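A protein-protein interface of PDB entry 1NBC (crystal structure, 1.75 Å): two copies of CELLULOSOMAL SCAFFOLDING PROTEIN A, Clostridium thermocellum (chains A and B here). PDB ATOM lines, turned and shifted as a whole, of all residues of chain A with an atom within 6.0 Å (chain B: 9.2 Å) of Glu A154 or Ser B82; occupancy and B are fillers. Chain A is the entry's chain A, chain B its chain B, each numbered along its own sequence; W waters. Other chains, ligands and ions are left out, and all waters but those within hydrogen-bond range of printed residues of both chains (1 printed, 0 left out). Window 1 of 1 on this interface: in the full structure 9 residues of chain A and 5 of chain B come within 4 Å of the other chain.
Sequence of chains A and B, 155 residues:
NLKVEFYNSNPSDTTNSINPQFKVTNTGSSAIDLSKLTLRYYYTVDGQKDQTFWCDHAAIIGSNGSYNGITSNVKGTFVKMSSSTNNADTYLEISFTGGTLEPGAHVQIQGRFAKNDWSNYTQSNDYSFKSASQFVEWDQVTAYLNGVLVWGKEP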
ATOM      1  N   ARG A  40     -20.470   6.650  -9.323  1.00  0.00           N
ATOM      2  CA  ARG A  40     -21.313   6.223 -10.437  1.00  0.00           C
ATOM      3  C   ARG A  40     -20.750   6.608 -11.798  1.00  0.00           C
ATOM      4  O   ARG A  40     -20.182   7.688 -11.983  1.00  0.00           O
ATOM      5  CB  ARG A  40     -22.744   6.776 -10.322  1.00  0.00           C
ATOM      6  CG  ARG A  40     -23.560   6.239  -9.185  1.00  0.00           C
ATOM      7  CD  ARG A  40     -24.926   6.831  -9.240  1.00  0.00           C
ATOM      8  NE  ARG A  40     -25.588   6.706  -7.952  1.00  0.00           N
ATOM      9  CZ  ARG A  40     -26.817   7.146  -7.684  1.00  0.00           C
ATOM     10  NH1 ARG A  40     -27.548   7.739  -8.619  1.00  0.00           N
ATOM     11  NH2 ARG A  40     -27.292   7.037  -6.459  1.00  0.00           N
ATOM     12  N   TYR A  42     -22.230   6.693 -15.602  1.00  0.00           N
ATOM     13  CA  TYR A  42     -23.450   6.633 -16.423  1.00  0.00           C
ATOM     14  C   TYR A  42     -23.190   6.369 -17.902  1.00  0.00           C
ATOM     15  O   TYR A  42     -22.284   6.956 -18.511  1.00  0.00           O
ATOM     16  CB  TYR A  42     -24.251   7.946 -16.311  1.00  0.00           C
ATOM     17  CG  TYR A  42     -24.800   8.268 -14.930  1.00  0.00           C
ATOM     18  CD1 TYR A  42     -24.016   8.943 -13.984  1.00  0.00           C
ATOM     19  CD2 TYR A  42     -26.106   7.912 -14.570  1.00  0.00           C
ATOM     20  CE1 TYR A  42     -24.518   9.255 -12.719  1.00  0.00           C
ATOM     21  CE2 TYR A  42     -26.620   8.224 -13.294  1.00  0.00           C
ATOM     22  CZ  TYR A  42     -25.815   8.893 -12.387  1.00  0.00           C
ATOM     23  OH  TYR A  42     -26.301   9.207 -11.147  1.00  0.00           O
ATOM     24  N   TYR A 127     -22.733   8.947 -21.258  1.00  0.00           N
ATOM     25  CA  TYR A 127     -22.613  10.178 -20.487  1.00  0.00           C
ATOM     26  C   TYR A 127     -21.286  10.372 -19.773  1.00  0.00           C
ATOM     27  O   TYR A 127     -20.704  11.452 -19.838  1.00  0.00           O
ATOM     28  CB  TYR A 127     -23.743  10.245 -19.454  1.00  0.00           C
ATOM     29  CG  TYR A 127     -23.739  11.505 -18.610  1.00  0.00           C
ATOM     30  CD1 TYR A 127     -24.214  12.724 -19.126  1.00  0.00           C
ATOM     31  CD2 TYR A 127     -23.270  11.484 -17.287  1.00  0.00           C
ATOM     32  CE1 TYR A 127     -24.218  13.894 -18.339  1.00  0.00           C
ATOM     33  CE2 TYR A 127     -23.267  12.644 -16.494  1.00  0.00           C
ATOM     34  CZ  TYR A 127     -23.745  13.847 -17.025  1.00  0.00           C
ATOM     35  OH  TYR A 127     -23.743  14.988 -16.251  1.00  0.00           O
ATOM     36  N   ASP A 139     -16.577  16.109 -14.259  1.00  0.00           N
ATOM     37  CA  ASP A 139     -17.816  16.193 -13.480  1.00  0.00           C
ATOM     38  C   ASP A 139     -18.979  15.390 -14.034  1.00  0.00           C
ATOM     39  O   ASP A 139     -20.114  15.588 -13.610  1.00  0.00           O
ATOM     40  CB  ASP A 139     -18.235  17.650 -13.247  1.00  0.00           C
ATOM     41  CG  ASP A 139     -18.672  18.346 -14.512  1.00  0.00           C
ATOM     42  OD1 ASP A 139     -18.434  17.836 -15.632  1.00  0.00           O
ATOM     43  OD2 ASP A 139     -19.259  19.435 -14.379  1.00  0.00           O
ATOM     44  N   THR A 142     -20.195  10.786 -10.837  1.00  0.00           N
ATOM     45  CA  THR A 142     -20.627  11.273  -9.536  1.00  0.00           C
ATOM     46  C   THR A 142     -20.133  10.447  -8.336  1.00  0.00           C
ATOM     47  O   THR A 142     -19.790   9.268  -8.464  1.00  0.00           O
ATOM     48  CB  THR A 142     -22.147  11.382  -9.514  1.00  0.00           C
ATOM     49  OG1 THR A 142     -22.702  10.123  -9.904  1.00  0.00           O
ATOM     50  CG2 THR A 142     -22.613  12.439 -10.506  1.00  0.00           C
ATOM     51  N   TYR A 144     -20.882   9.951  -3.904  1.00  0.00           N
ATOM     52  CA  TYR A 144     -21.854  10.162  -2.839  1.00  0.00           C
ATOM     53  C   TYR A 144     -21.314   9.730  -1.492  1.00  0.00           C
ATOM     54  O   TYR A 144     -20.567   8.767  -1.411  1.00  0.00           O
ATOM     55  CB  TYR A 144     -23.128   9.352  -3.118  1.00  0.00           C
ATOM     56  CG  TYR A 144     -23.681   9.570  -4.493  1.00  0.00           C
ATOM     57  CD1 TYR A 144     -23.096   8.956  -5.601  1.00  0.00           C
ATOM     58  CD2 TYR A 144     -24.758  10.428  -4.702  1.00  0.00           C
ATOM     59  CE1 TYR A 144     -23.560   9.195  -6.876  1.00  0.00           C
ATOM     60  CE2 TYR A 144     -25.234  10.677  -5.977  1.00  0.00           C
ATOM     61  CZ  TYR A 144     -24.628  10.059  -7.066  1.00  0.00           C
ATOM     62  OH  TYR A 144     -25.065  10.317  -8.346  1.00  0.00           O
ATOM     63  N   GLY A 147     -25.306   8.377   0.468  1.00  0.00           N
ATOM     64  CA  GLY A 147     -26.398   8.703  -0.435  1.00  0.00           C
ATOM     65  C   GLY A 147     -26.512  10.156  -0.868  1.00  0.00           C
ATOM     66  O   GLY A 147     -27.345  10.472  -1.713  1.00  0.00           O
ATOM     67  N   VAL A 148     -25.710  11.049  -0.306  1.00  0.00           N
ATOM     68  CA  VAL A 148     -25.771  12.443  -0.703  1.00  0.00           C
ATOM     69  C   VAL A 148     -24.729  12.727  -1.770  1.00  0.00           C
ATOM     70  O   VAL A 148     -23.573  12.331  -1.621  1.00  0.00           O
ATOM     71  CB  VAL A 148     -25.514  13.360   0.491  1.00  0.00           C
ATOM     72  CG1 VAL A 148     -25.411  14.827   0.040  1.00  0.00           C
ATOM     73  CG2 VAL A 148     -26.617  13.170   1.518  1.00  0.00           C
ATOM     74  N   LEU A 149     -25.145  13.395  -2.847  1.00  0.00           N
ATOM     75  CA  LEU A 149     -24.245  13.755  -3.950  1.00  0.00           C
ATOM     76  C   LEU A 149     -23.245  14.790  -3.479  1.00  0.00           C
ATOM     77  O   LEU A 149     -23.636  15.855  -3.008  1.00  0.00           O
ATOM     78  CB  LEU A 149     -25.023  14.349  -5.118  1.00  0.00           C
ATOM     79  CG  LEU A 149     -24.208  14.883  -6.301  1.00  0.00           C
ATOM     80  CD1 LEU A 149     -23.725  13.728  -7.126  1.00  0.00           C
ATOM     81  CD2 LEU A 149     -25.060  15.785  -7.165  1.00  0.00           C
ATOM     82  N   GLY A 152     -19.829  15.934  -8.943  1.00  0.00           N
ATOM     83  CA  GLY A 152     -20.334  15.672 -10.278  1.00  0.00           C
ATOM     84  C   GLY A 152     -21.739  16.108 -10.564  1.00  0.00           C
ATOM     85  O   GLY A 152     -22.465  16.552  -9.676  1.00  0.00           O
ATOM     86  N   LYS A 153     -22.104  15.990 -11.828  1.00  0.00           N
ATOM     87  CA  LYS A 153     -23.419  16.356 -12.307  1.00  0.00           C
ATOM     88  C   LYS A 153     -24.144  15.101 -12.738  1.00  0.00           C
ATOM     89  O   LYS A 153     -23.634  14.331 -13.554  1.00  0.00           O
ATOM     90  CB  LYS A 153     -23.308  17.260 -13.539  1.00  0.00           C
ATOM     91  CG  LYS A 153     -22.703  18.630 -13.310  1.00  0.00           C
ATOM     92  CD  LYS A 153     -22.711  19.433 -14.616  1.00  0.00           C
ATOM     93  CE  LYS A 153     -22.629  20.941 -14.364  1.00  0.00           C
ATOM     94  NZ  LYS A 153     -21.486  21.325 -13.470  1.00  0.00           N
ATOM     95  N   GLU A 154     -25.318  14.866 -12.180  1.00  0.00           N
ATOM     96  CA  GLU A 154     -26.085  13.700 -12.593  1.00  0.00           C
ATOM     97  C   GLU A 154     -26.741  14.023 -13.920  1.00  0.00           C
ATOM     98  O   GLU A 154     -26.938  15.203 -14.241  1.00  0.00           O
ATOM     99  CB  GLU A 154     -27.141  13.349 -11.561  1.00  0.00           C
ATOM    100  CG  GLU A 154     -26.573  12.734 -10.329  1.00  0.00           C
ATOM    101  CD  GLU A 154     -27.633  12.420  -9.330  1.00  0.00           C
ATOM    102  OE1 GLU A 154     -28.721  13.027  -9.384  1.00  0.00           O
ATOM    103  OE2 GLU A 154     -27.384  11.559  -8.474  1.00  0.00           O
ATOM    104  N   PRO A 155     -26.965  13.008 -14.759  1.00  0.00           N
ATOM    105  CA  PRO A 155     -27.601  13.301 -16.045  1.00  0.00           C
ATOM    106  C   PRO A 155     -29.034  13.785 -15.854  1.00  0.00           C
ATOM    107  O   PRO A 155     -29.697  13.327 -14.901  1.00  0.00           O
ATOM    108  CB  PRO A 155     -27.524  11.962 -16.791  1.00  0.00           C
ATOM    109  CG  PRO A 155     -27.331  10.927 -15.695  1.00  0.00           C
ATOM    110  CD  PRO A 155     -26.464  11.622 -14.703  1.00  0.00           C
ATOM    111  N   ARG B  40     -44.583  10.293  -9.394  1.00  0.00           N
ATOM    112  CA  ARG B  40     -43.805  10.787  -8.259  1.00  0.00           C
ATOM    113  C   ARG B  40     -44.425  12.011  -7.577  1.00  0.00           C
ATOM    114  O   ARG B  40     -45.052  12.859  -8.218  1.00  0.00           O
ATOM    115  CB  ARG B  40     -42.373  11.121  -8.668  1.00  0.00           C
ATOM    116  CG  ARG B  40     -41.575   9.946  -9.173  1.00  0.00           C
ATOM    117  CD  ARG B  40     -40.165  10.382  -9.475  1.00  0.00           C
ATOM    118  NE  ARG B  40     -39.451   9.370 -10.240  1.00  0.00           N
ATOM    119  CZ  ARG B  40     -38.197   9.493 -10.662  1.00  0.00           C
ATOM    120  NH1 ARG B  40     -37.496  10.586 -10.397  1.00  0.00           N
ATOM    121  NH2 ARG B  40     -37.653   8.520 -11.368  1.00  0.00           N
ATOM    122  N   TYR B  42     -43.014  14.772  -4.934  1.00  0.00           N
ATOM    123  CA  TYR B  42     -41.815  15.340  -4.295  1.00  0.00           C
ATOM    124  C   TYR B  42     -42.119  16.184  -3.070  1.00  0.00           C
ATOM    125  O   TYR B  42     -43.044  17.008  -3.071  1.00  0.00           O
ATOM    126  CB  TYR B  42     -41.035  16.211  -5.297  1.00  0.00           C
ATOM    127  CG  TYR B  42     -40.460  15.459  -6.485  1.00  0.00           C
ATOM    128  CD1 TYR B  42     -41.218  15.242  -7.642  1.00  0.00           C
ATOM    129  CD2 TYR B  42     -39.150  14.966  -6.454  1.00  0.00           C
ATOM    130  CE1 TYR B  42     -40.678  14.548  -8.742  1.00  0.00           C
ATOM    131  CE2 TYR B  42     -38.598  14.269  -7.544  1.00  0.00           C
ATOM    132  CZ  TYR B  42     -39.364  14.066  -8.679  1.00  0.00           C
ATOM    133  OH  TYR B  42     -38.803  13.382  -9.734  1.00  0.00           O
ATOM    134  N   VAL B  79     -38.177   7.130  -2.015  1.00  0.00           N
ATOM    135  CA  VAL B  79     -36.819   7.311  -2.500  1.00  0.00           C
ATOM    136  C   VAL B  79     -36.199   8.614  -1.987  1.00  0.00           C
ATOM    137  O   VAL B  79     -36.756   9.692  -2.178  1.00  0.00           O
ATOM    138  CB  VAL B  79     -36.811   7.327  -4.062  1.00  0.00           C
ATOM    139  CG1 VAL B  79     -35.397   7.420  -4.582  1.00  0.00           C
ATOM    140  CG2 VAL B  79     -37.515   6.091  -4.627  1.00  0.00           C
ATOM    141  N   LYS B  80     -35.077   8.508  -1.291  1.00  0.00           N
ATOM    142  CA  LYS B  80     -34.401   9.696  -0.807  1.00  0.00           C
ATOM    143  C   LYS B  80     -33.524  10.241  -1.940  1.00  0.00           C
ATOM    144  O   LYS B  80     -32.706   9.517  -2.502  1.00  0.00           O
ATOM    145  CB  LYS B  80     -33.572   9.384   0.442  1.00  0.00           C
ATOM    146  CG  LYS B  80     -32.803  10.590   0.961  1.00  0.00           C
ATOM    147  CD  LYS B  80     -32.323  10.388   2.383  1.00  0.00           C
ATOM    148  CE  LYS B  80     -31.098  11.243   2.662  1.00  0.00           C
ATOM    149  NZ  LYS B  80     -29.919  10.768   1.864  1.00  0.00           N
ATOM    150  N   MET B  81     -33.742  11.497  -2.305  1.00  0.00           N
ATOM    151  CA  MET B  81     -33.004  12.135  -3.385  1.00  0.00           C
ATOM    152  C   MET B  81     -31.528  12.357  -3.016  1.00  0.00           C
ATOM    153  O   MET B  81     -31.215  12.769  -1.903  1.00  0.00           O
ATOM    154  CB  MET B  81     -33.674  13.468  -3.735  1.00  0.00           C
ATOM    155  CG  MET B  81     -35.108  13.317  -4.230  1.00  0.00           C
ATOM    156  SD  MET B  81     -35.996  14.868  -4.229  1.00  0.00           S
ATOM    157  CE  MET B  81     -35.055  15.776  -5.400  1.00  0.00           C
ATOM    158  N   SER B  82     -30.629  12.097  -3.963  1.00  0.00           N
ATOM    159  CA  SER B  82     -29.191  12.282  -3.732  1.00  0.00           C
ATOM    160  C   SER B  82     -28.862  13.774  -3.687  1.00  0.00           C
ATOM    161  O   SER B  82     -27.963  14.217  -2.965  1.00  0.00           O
ATOM    162  CB  SER B  82     -28.400  11.607  -4.837  1.00  0.00           C
ATOM    163  OG  SER B  82     -28.781  12.151  -6.079  1.00  0.00           O
ATOM    164  N   SER B  83     -29.601  14.531  -4.490  1.00  0.00           N
ATOM    165  CA  SER B  83     -29.472  15.976  -4.563  1.00  0.00           C
ATOM    166  C   SER B  83     -30.856  16.594  -4.262  1.00  0.00           C
ATOM    167  O   SER B  83     -31.832  16.371  -4.989  1.00  0.00           O
ATOM    168  CB  SER B  83     -28.977  16.372  -5.957  1.00  0.00           C
ATOM    169  OG  SER B  83     -28.391  17.662  -5.941  1.00  0.00           O
ATOM    170  N   SER B  84     -30.939  17.343  -3.172  1.00  0.00           N
ATOM    171  CA  SER B  84     -32.193  17.949  -2.753  1.00  0.00           C
ATOM    172  C   SER B  84     -32.250  19.462  -2.965  1.00  0.00           C
ATOM    173  O   SER B  84     -31.227  20.125  -3.156  1.00  0.00           O
ATOM    174  CB  SER B  84     -32.434  17.645  -1.279  1.00  0.00           C
ATOM    175  OG  SER B  84     -31.634  18.472  -0.445  1.00  0.00           O
ATOM    176  N   THR B  85     -33.468  19.994  -2.912  1.00  0.00           N
ATOM    177  CA  THR B  85     -33.738  21.418  -3.068  1.00  0.00           C
ATOM    178  C   THR B  85     -34.415  21.888  -1.781  1.00  0.00           C
ATOM    179  O   THR B  85     -34.657  21.070  -0.889  1.00  0.00           O
ATOM    180  CB  THR B  85     -34.646  21.688  -4.297  1.00  0.00           C
ATOM    181  OG1 THR B  85     -35.935  21.100  -4.101  1.00  0.00           O
ATOM    182  CG2 THR B  85     -34.035  21.083  -5.541  1.00  0.00           C
ATOM    183  N   ALA B  88     -37.688  19.761  -1.738  1.00  0.00           N
ATOM    184  CA  ALA B  88     -37.701  18.373  -2.208  1.00  0.00           C
ATOM    185  C   ALA B  88     -36.445  17.591  -1.844  1.00  0.00           C
ATOM    186  O   ALA B  88     -35.372  17.875  -2.359  1.00  0.00           O
ATOM    187  CB  ALA B  88     -37.924  18.309  -3.705  1.00  0.00           C
ATOM    188  N   ASP B  89     -36.576  16.613  -0.948  1.00  0.00           N
ATOM    189  CA  ASP B  89     -35.445  15.764  -0.583  1.00  0.00           C
ATOM    190  C   ASP B  89     -35.820  14.294  -0.632  1.00  0.00           C
ATOM    191  O   ASP B  89     -34.968  13.432  -0.526  1.00  0.00           O
ATOM    192  CB  ASP B  89     -34.849  16.137   0.785  1.00  0.00           C
ATOM    193  CG  ASP B  89     -35.855  16.088   1.914  1.00  0.00           C
ATOM    194  OD1 ASP B  89     -36.858  15.341   1.811  1.00  0.00           O
ATOM    195  OD2 ASP B  89     -35.624  16.776   2.939  1.00  0.00           O
ATOM    196  N   THR B  90     -37.099  14.027  -0.876  1.00  0.00           N
ATOM    197  CA  THR B  90     -37.632  12.667  -0.939  1.00  0.00           C
ATOM    198  C   THR B  90     -38.805  12.610  -1.911  1.00  0.00           C
ATOM    199  O   THR B  90     -39.432  13.643  -2.188  1.00  0.00           O
ATOM    200  CB  THR B  90     -38.235  12.272   0.421  1.00  0.00           C
ATOM    201  OG1 THR B  90     -37.308  12.563   1.467  1.00  0.00           O
ATOM    202  CG2 THR B  90     -38.590  10.810   0.453  1.00  0.00           C
ATOM    203  N   TYR B  91     -39.075  11.441  -2.478  1.00  0.00           N
ATOM    204  CA  TYR B  91     -40.256  11.313  -3.314  1.00  0.00           C
ATOM    205  C   TYR B  91     -40.907   9.962  -3.162  1.00  0.00           C
ATOM    206  O   TYR B  91     -40.259   8.965  -2.813  1.00  0.00           O
ATOM    207  CB  TYR B  91     -39.972  11.561  -4.826  1.00  0.00           C
ATOM    208  CG  TYR B  91     -39.074  10.603  -5.590  1.00  0.00           C
ATOM    209  CD1 TYR B  91     -39.520   9.345  -5.993  1.00  0.00           C
ATOM    210  CD2 TYR B  91     -37.774  10.970  -5.923  1.00  0.00           C
ATOM    211  CE1 TYR B  91     -38.691   8.491  -6.700  1.00  0.00           C
ATOM    212  CE2 TYR B  91     -36.946  10.125  -6.624  1.00  0.00           C
ATOM    213  CZ  TYR B  91     -37.401   8.893  -7.010  1.00  0.00           C
ATOM    214  OH  TYR B  91     -36.550   8.059  -7.694  1.00  0.00           O
ATOM    215  N   PRO B 155     -37.975  18.667  -9.868  1.00  0.00           N
ATOM    216  CA  PRO B 155     -37.316  19.762  -9.157  1.00  0.00           C
ATOM    217  C   PRO B 155     -35.820  19.815  -9.473  1.00  0.00           C
ATOM    218  O   PRO B 155     -35.208  18.742  -9.642  1.00  0.00           O
ATOM    219  CB  PRO B 155     -37.595  19.443  -7.681  1.00  0.00           C
ATOM    220  CG  PRO B 155     -37.785  17.957  -7.668  1.00  0.00           C
ATOM    221  CD  PRO B 155     -38.531  17.669  -8.937  1.00  0.00           C
HETATM  222  O   HOH W   1     -29.838   9.879  -7.341  1.00  0.00           O
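Positions printed for both chains: 40, 42 and 155.
Of the 5 pairs that touch across the chains among the printed residues, none has its exchanged pair printed and touching as well.
Thr A142 touches none of the printed residues of chain B.
Of the printed residues of chain B, Tyr A144 touches Ser B82 (3.5 Å).
Of the printed residues of chain B, Gly A147 touches Ser B82.
Of the printed residues of chain B, Leu A149 touches Ser B82 (2.9 Å).
Glu A154 touches one residue of chain B.
Pro A155 touches none of the printed residues of chain B.
Of chain A, only Tyr A144, Gly A147, Val A148, Leu A149 and Glu A154 come within 4 Å of Ser B82.
Ser B84 touches none of the printed residues of chain A.
The nearest residue of chain A that does not touch Ser B82 is Arg A40 (5.0 Å).
The backbone carbonyl oxygen (O) of Ser B82 is in hydrogen-bond range of the backbone NH (N) of Leu A149.
The side-chain hydroxyl of Ser B82 sits at hydrogen-bond distance from the side-chain carboxylate of Glu A154 (2.8 Å).
Water W1 lies within hydrogen-bond range of OG of Ser B82, OE2 of Glu A154 and NH1 of Arg A40.
Tyr A144 touches Ser B82 (CE2 to CB, 3.5 Å).
Gly A147 touches Ser B82 (O to CA, 3.3 Å).
Val A148 touches Ser B82 (CA to O, 3.6 Å).
Hydrophobic or aromatic side chains of chain A that line the printed part of chain B: Tyr A144, Val A148 and Leu A149.
Among the printed residues, no Asp or Glu carboxylate lies within 4 Å of a Lys or Arg side-chain nitrogen of the other chain.
NH1 of Arg A40 lies within salt-bridge range of OE2 of Glu A154, at 3.8 Å.
OH of Tyr A42 sits at hydrogen-bond distance from OH of Tyr A144.
OG1 of Thr A142 sits at hydrogen-bond distance from OH of Tyr A144, 2.8 Å away.
The side-chain carboxylate (OE2) of Glu A154 sits at hydrogen-bond distance from the side-chain hydroxyl (OH) of Tyr A144, at 2.6 Å.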
